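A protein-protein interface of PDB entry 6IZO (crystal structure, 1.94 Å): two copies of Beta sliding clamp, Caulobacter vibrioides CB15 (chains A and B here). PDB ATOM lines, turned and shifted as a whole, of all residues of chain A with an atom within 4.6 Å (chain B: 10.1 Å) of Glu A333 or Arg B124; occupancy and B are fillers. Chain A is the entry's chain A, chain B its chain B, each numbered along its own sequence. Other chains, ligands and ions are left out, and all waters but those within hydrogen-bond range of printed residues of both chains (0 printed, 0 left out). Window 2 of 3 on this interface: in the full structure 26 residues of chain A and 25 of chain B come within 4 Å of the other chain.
Among the printed residues, merely in contact across the chains: Val A329 with Arg B124, Val A329 with Ser B125, Glu A330 with Arg B124 and Glu A333 with Arg B124.
Along chain A the printed residues that touch a printed residue of chain B span positions 329 to 333.
No position is printed for both chains. Of the 7 pairs that touch across the chains among the printed residues, none has its exchanged pair printed and touching as well.
The guanidinium group (NH2) of Arg A315 is in salt-bridge range of the side-chain carboxylate (OE2) of Glu A331, at 3.2 Å. The side-chain amide nitrogen of Gln B121 sits at hydrogen-bond distance from the backbone carbonyl oxygen of Ser B125 (3.1 Å).
The backbone carbonyl oxygen (O) of Val A329 lies within hydrogen-bond range of the backbone NH (N) of Arg B126 (2.9 Å). OE1 of Glu A330 sits at hydrogen-bond distance from OG of Ser B125 (2.7 Å). The guanidinium group (NH2) of Arg B124 is in salt-bridge range of the side-chain carboxylate (OE1) of Glu A331, at 3.98 Å.
Glu A333 touches just one residue of chain B: Arg B124 (3.6 Å). Arg B124 touches four residues of chain A. Of chain B, only Arg B124 (3.4 Å) and Ser B125 (2.7 Å) come within 4 Å of Glu A330. Of chain B, only Arg B124 (3.4 Å) comes within 4 Å of Glu A331. No residue of chain B comes within 4 Å of Val A332. No residue of chain B comes within 4 Å of Val A334. Printed residues of chain A within 4 Å of Arg B126: Val A329 (2.9 Å). Printed residues of chain B within 4 Å of Val A329: Arg B124, Ser B125 and Arg B126. Of the printed residues of chain A, Ser B125 touches Val A329 (3.5 Å) and Glu A330 (2.7 Å). Ala B122 touches none of the printed residues of chain A. The nearest printed residue of chain B that does not touch Glu A333 is Gly B123 (10.1 Å). The nearest printed residue of chain A that does not touch Arg B124 is Arg A315 (4.1 Å). The nearest printed residue of chain A that does not touch Arg B126 is Glu A330 (5.1 Å).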
ATOM      1  N   GLY A 314     -19.263 -16.627  37.147  1.00  0.00           N
ATOM      2  CA  GLY A 314     -18.656 -16.717  35.823  1.00  0.00           C
ATOM      3  C   GLY A 314     -17.454 -15.810  35.560  1.00  0.00           C
ATOM      4  O   GLY A 314     -16.827 -15.942  34.519  1.00  0.00           O
ATOM      5  N   ARG A 315     -17.082 -14.908  36.470  1.00  0.00           N
ATOM      6  CA  ARG A 315     -16.102 -13.888  36.074  1.00  0.00           C
ATOM      7  C   ARG A 315     -15.343 -13.238  37.210  1.00  0.00           C
ATOM      8  O   ARG A 315     -15.908 -12.971  38.250  1.00  0.00           O
ATOM      9  CB  ARG A 315     -16.857 -12.821  35.261  1.00  0.00           C
ATOM     10  CG  ARG A 315     -16.075 -11.593  34.849  1.00  0.00           C
ATOM     11  CD  ARG A 315     -16.971 -10.644  34.065  1.00  0.00           C
ATOM     12  NE  ARG A 315     -17.446 -11.248  32.821  1.00  0.00           N
ATOM     13  CZ  ARG A 315     -18.334 -10.694  31.995  1.00  0.00           C
ATOM     14  NH1 ARG A 315     -18.684 -11.338  30.885  1.00  0.00           N
ATOM     15  NH2 ARG A 315     -18.867  -9.499  32.259  1.00  0.00           N
ATOM     16  N   VAL A 329      -7.634  -2.879  33.108  1.00  0.00           N
ATOM     17  CA  VAL A 329      -8.786  -3.715  33.447  1.00  0.00           C
ATOM     18  C   VAL A 329      -8.774  -4.914  32.523  1.00  0.00           C
ATOM     19  O   VAL A 329      -8.543  -4.779  31.315  1.00  0.00           O
ATOM     20  CB  VAL A 329     -10.136  -2.974  33.315  1.00  0.00           C
ATOM     21  CG1 VAL A 329     -11.309  -3.898  33.658  1.00  0.00           C
ATOM     22  CG2 VAL A 329     -10.174  -1.754  34.222  1.00  0.00           C
ATOM     23  N   GLU A 330      -9.037  -6.084  33.088  1.00  0.00           N
ATOM     24  CA  GLU A 330      -9.199  -7.294  32.289  1.00  0.00           C
ATOM     25  C   GLU A 330     -10.219  -8.234  32.932  1.00  0.00           C
ATOM     26  O   GLU A 330     -10.195  -8.439  34.148  1.00  0.00           O
ATOM     27  CB  GLU A 330      -7.862  -8.004  32.095  1.00  0.00           C
ATOM     28  CG  GLU A 330      -7.944  -9.221  31.170  1.00  0.00           C
ATOM     29  CD  GLU A 330      -6.613  -9.657  30.584  1.00  0.00           C
ATOM     30  OE1 GLU A 330      -5.619  -8.899  30.600  1.00  0.00           O
ATOM     31  OE2 GLU A 330      -6.543 -10.786  30.095  1.00  0.00           O
ATOM     32  N   GLU A 331     -11.080  -8.819  32.100  1.00  0.00           N
ATOM     33  CA  GLU A 331     -12.078  -9.777  32.549  1.00  0.00           C
ATOM     34  C   GLU A 331     -11.549 -11.161  32.250  1.00  0.00           C
ATOM     35  O   GLU A 331     -10.991 -11.389  31.181  1.00  0.00           O
ATOM     36  CB  GLU A 331     -13.404  -9.540  31.824  1.00  0.00           C
ATOM     37  CG  GLU A 331     -14.060  -8.211  32.189  1.00  0.00           C
ATOM     38  CD  GLU A 331     -15.256  -7.877  31.307  1.00  0.00           C
ATOM     39  OE1 GLU A 331     -15.109  -7.893  30.067  1.00  0.00           O
ATOM     40  OE2 GLU A 331     -16.339  -7.594  31.856  1.00  0.00           O
ATOM     41  N   VAL A 332     -11.682 -12.065  33.222  1.00  0.00           N
ATOM     42  CA  VAL A 332     -11.275 -13.464  33.056  1.00  0.00           C
ATOM     43  C   VAL A 332     -12.466 -14.329  33.448  1.00  0.00           C
ATOM     44  O   VAL A 332     -13.065 -14.128  34.498  1.00  0.00           O
ATOM     45  CB  VAL A 332     -10.056 -13.828  33.945  1.00  0.00           C
ATOM     46  CG1 VAL A 332      -9.678 -15.293  33.797  1.00  0.00           C
ATOM     47  CG2 VAL A 332      -8.871 -12.945  33.577  1.00  0.00           C
ATOM     48  N   GLU A 333     -12.796 -15.290  32.595  1.00  0.00           N
ATOM     49  CA  GLU A 333     -13.835 -16.256  32.895  1.00  0.00           C
ATOM     50  C   GLU A 333     -13.340 -17.230  33.977  1.00  0.00           C
ATOM     51  O   GLU A 333     -12.224 -17.712  33.914  1.00  0.00           O
ATOM     52  CB  GLU A 333     -14.235 -17.001  31.616  1.00  0.00           C
ATOM     53  CG  GLU A 333     -14.814 -16.085  30.533  1.00  0.00           C
ATOM     54  CD  GLU A 333     -14.991 -16.785  29.184  1.00  0.00           C
ATOM     55  OE1 GLU A 333     -14.739 -18.008  29.079  1.00  0.00           O
ATOM     56  OE2 GLU A 333     -15.393 -16.114  28.212  1.00  0.00           O
ATOM     57  N   VAL A 334     -14.149 -17.457  35.000  1.00  0.00           N
ATOM     58  CA  VAL A 334     -13.834 -18.413  36.067  1.00  0.00           C
ATOM     59  C   VAL A 334     -15.065 -19.256  36.387  1.00  0.00           C
ATOM     60  O   VAL A 334     -16.169 -18.940  35.956  1.00  0.00           O
ATOM     61  CB  VAL A 334     -13.344 -17.715  37.364  1.00  0.00           C
ATOM     62  CG1 VAL A 334     -12.158 -16.786  37.074  1.00  0.00           C
ATOM     63  CG2 VAL A 334     -14.467 -16.954  38.051  1.00  0.00           C
ATOM     64  N   LEU B 101       0.505  -8.701  25.701  1.00  0.00           N
ATOM     65  CA  LEU B 101      -0.753  -9.022  25.023  1.00  0.00           C
ATOM     66  C   LEU B 101      -0.579 -10.371  24.307  1.00  0.00           C
ATOM     67  O   LEU B 101       0.538 -10.713  23.945  1.00  0.00           O
ATOM     68  CB  LEU B 101      -1.137  -7.940  24.000  1.00  0.00           C
ATOM     69  CG  LEU B 101      -1.601  -6.574  24.506  1.00  0.00           C
ATOM     70  CD1 LEU B 101      -1.931  -5.669  23.333  1.00  0.00           C
ATOM     71  CD2 LEU B 101      -2.790  -6.685  25.448  1.00  0.00           C
ATOM     72  N   PRO B 102      -1.671 -11.134  24.112  1.00  0.00           N
ATOM     73  CA  PRO B 102      -1.553 -12.437  23.431  1.00  0.00           C
ATOM     74  C   PRO B 102      -0.973 -12.319  22.026  1.00  0.00           C
ATOM     75  O   PRO B 102      -1.130 -11.275  21.386  1.00  0.00           O
ATOM     76  CB  PRO B 102      -3.000 -12.931  23.336  1.00  0.00           C
ATOM     77  CG  PRO B 102      -3.758 -12.167  24.347  1.00  0.00           C
ATOM     78  CD  PRO B 102      -3.042 -10.870  24.576  1.00  0.00           C
ATOM     79  N   ALA B 105      -2.670 -10.606  18.646  1.00  0.00           N
ATOM     80  CA  ALA B 105      -3.671  -9.632  19.067  1.00  0.00           C
ATOM     81  C   ALA B 105      -3.691  -8.402  18.152  1.00  0.00           C
ATOM     82  O   ALA B 105      -2.643  -7.880  17.764  1.00  0.00           O
ATOM     83  CB  ALA B 105      -3.426  -9.203  20.500  1.00  0.00           C
ATOM     84  N   ASP B 106      -4.892  -7.963  17.804  1.00  0.00           N
ATOM     85  CA  ASP B 106      -5.075  -6.703  17.093  1.00  0.00           C
ATOM     86  C   ASP B 106      -5.285  -5.641  18.139  1.00  0.00           C
ATOM     87  O   ASP B 106      -6.110  -5.818  19.017  1.00  0.00           O
ATOM     88  CB  ASP B 106      -6.242  -6.787  16.111  1.00  0.00           C
ATOM     89  CG  ASP B 106      -5.805  -7.326  14.767  1.00  0.00           C
ATOM     90  OD1 ASP B 106      -5.510  -6.502  13.866  1.00  0.00           O
ATOM     91  OD2 ASP B 106      -5.691  -8.562  14.633  1.00  0.00           O
ATOM     92  N   VAL B 107      -4.515  -4.558  18.065  1.00  0.00           N
ATOM     93  CA  VAL B 107      -4.480  -3.563  19.141  1.00  0.00           C
ATOM     94  C   VAL B 107      -5.126  -2.265  18.684  1.00  0.00           C
ATOM     95  O   VAL B 107      -4.660  -1.652  17.714  1.00  0.00           O
ATOM     96  CB  VAL B 107      -3.040  -3.268  19.592  1.00  0.00           C
ATOM     97  CG1 VAL B 107      -3.032  -2.341  20.806  1.00  0.00           C
ATOM     98  CG2 VAL B 107      -2.286  -4.563  19.881  1.00  0.00           C
ATOM     99  N   ILE B 120      -5.838   1.784  25.201  1.00  0.00           N
ATOM    100  CA  ILE B 120      -5.277   0.647  24.498  1.00  0.00           C
ATOM    101  C   ILE B 120      -6.179  -0.528  24.797  1.00  0.00           C
ATOM    102  O   ILE B 120      -6.361  -0.889  25.959  1.00  0.00           O
ATOM    103  CB  ILE B 120      -3.843   0.303  24.965  1.00  0.00           C
ATOM    104  CG1 ILE B 120      -2.916   1.521  24.800  1.00  0.00           C
ATOM    105  CG2 ILE B 120      -3.290  -0.884  24.187  1.00  0.00           C
ATOM    106  CD1 ILE B 120      -2.564   2.219  26.081  1.00  0.00           C
ATOM    107  N   GLN B 121      -6.694  -1.149  23.746  1.00  0.00           N
ATOM    108  CA  GLN B 121      -7.706  -2.189  23.885  1.00  0.00           C
ATOM    109  C   GLN B 121      -7.313  -3.321  22.966  1.00  0.00           C
ATOM    110  O   GLN B 121      -7.049  -3.094  21.790  1.00  0.00           O
ATOM    111  CB  GLN B 121      -9.080  -1.613  23.511  1.00  0.00           C
ATOM    112  CG  GLN B 121     -10.206  -2.626  23.321  1.00  0.00           C
ATOM    113  CD  GLN B 121     -11.039  -2.813  24.574  1.00  0.00           C
ATOM    114  OE1 GLN B 121     -11.754  -1.898  24.987  1.00  0.00           O
ATOM    115  NE2 GLN B 121     -10.958  -3.997  25.184  1.00  0.00           N
ATOM    116  N   ALA B 122      -7.271  -4.530  23.513  1.00  0.00           N
ATOM    117  CA  ALA B 122      -7.045  -5.756  22.755  1.00  0.00           C
ATOM    118  C   ALA B 122      -7.712  -6.926  23.477  1.00  0.00           C
ATOM    119  O   ALA B 122      -7.439  -7.138  24.662  1.00  0.00           O
ATOM    120  CB  ALA B 122      -5.560  -6.031  22.635  1.00  0.00           C
ATOM    121  N   GLY B 123      -8.552  -7.687  22.761  1.00  0.00           N
ATOM    122  CA  GLY B 123      -9.343  -8.785  23.345  1.00  0.00           C
ATOM    123  C   GLY B 123     -10.103  -8.302  24.561  1.00  0.00           C
ATOM    124  O   GLY B 123     -10.815  -7.301  24.493  1.00  0.00           O
ATOM    125  N   ARG B 124      -9.884  -8.956  25.696  1.00  0.00           N
ATOM    126  CA  ARG B 124     -10.550  -8.585  26.951  1.00  0.00           C
ATOM    127  C   ARG B 124      -9.725  -7.678  27.904  1.00  0.00           C
ATOM    128  O   ARG B 124     -10.103  -7.504  29.070  1.00  0.00           O
ATOM    129  CB  ARG B 124     -11.045  -9.868  27.643  1.00  0.00           C
ATOM    130  CG  ARG B 124     -12.311 -10.422  26.985  1.00  0.00           C
ATOM    131  CD  ARG B 124     -12.525 -11.926  27.167  1.00  0.00           C
ATOM    132  NE  ARG B 124     -12.994 -12.327  28.504  1.00  0.00           N
ATOM    133  CZ  ARG B 124     -14.219 -12.117  29.007  1.00  0.00           C
ATOM    134  NH1 ARG B 124     -14.508 -12.545  30.236  1.00  0.00           N
ATOM    135  NH2 ARG B 124     -15.158 -11.473  28.318  1.00  0.00           N
ATOM    136  N   SER B 125      -8.648  -7.074  27.398  1.00  0.00           N
ATOM    137  CA  SER B 125      -7.832  -6.103  28.153  1.00  0.00           C
ATOM    138  C   SER B 125      -8.087  -4.657  27.720  1.00  0.00           C
ATOM    139  O   SER B 125      -8.204  -4.386  26.531  1.00  0.00           O
ATOM    140  CB  SER B 125      -6.347  -6.391  27.947  1.00  0.00           C
ATOM    141  OG  SER B 125      -6.052  -7.744  28.192  1.00  0.00           O
ATOM    142  N   ARG B 126      -8.156  -3.738  28.683  1.00  0.00           N
ATOM    143  CA  ARG B 126      -8.288  -2.306  28.399  1.00  0.00           C
ATOM    144  C   ARG B 126      -7.354  -1.510  29.296  1.00  0.00           C
ATOM    145  O   ARG B 126      -7.370  -1.699  30.516  1.00  0.00           O
ATOM    146  CB  ARG B 126      -9.729  -1.840  28.622  1.00  0.00           C
ATOM    147  CG  ARG B 126     -10.044  -0.454  28.063  1.00  0.00           C
ATOM    148  CD  ARG B 126     -11.498  -0.098  28.330  1.00  0.00           C
ATOM    149  NE  ARG B 126     -11.954   1.094  27.617  1.00  0.00           N
ATOM    150  CZ  ARG B 126     -11.951   2.346  28.091  1.00  0.00           C
ATOM    151  NH1 ARG B 126     -12.417   3.333  27.329  1.00  0.00           N
ATOM    152  NH2 ARG B 126     -11.494   2.637  29.311  1.00  0.00           N
ATOM    153  N   PHE B 127      -6.538  -0.636  28.698  1.00  0.00           N
ATOM    154  CA  PHE B 127      -5.613   0.207  29.451  1.00  0.00           C
ATOM    155  C   PHE B 127      -5.864   1.673  29.126  1.00  0.00           C
ATOM    156  O   PHE B 127      -6.139   2.021  27.975  1.00  0.00           O
ATOM    157  CB  PHE B 127      -4.160  -0.123  29.131  1.00  0.00           C
ATOM    158  CG  PHE B 127      -3.796  -1.555  29.324  1.00  0.00           C
ATOM    159  CD1 PHE B 127      -4.141  -2.505  28.376  1.00  0.00           C
ATOM    160  CD2 PHE B 127      -3.079  -1.955  30.446  1.00  0.00           C
ATOM    161  CE1 PHE B 127      -3.802  -3.831  28.550  1.00  0.00           C
ATOM    162  CE2 PHE B 127      -2.736  -3.280  30.622  1.00  0.00           C
ATOM    163  CZ  PHE B 127      -3.089  -4.218  29.670  1.00  0.00           C
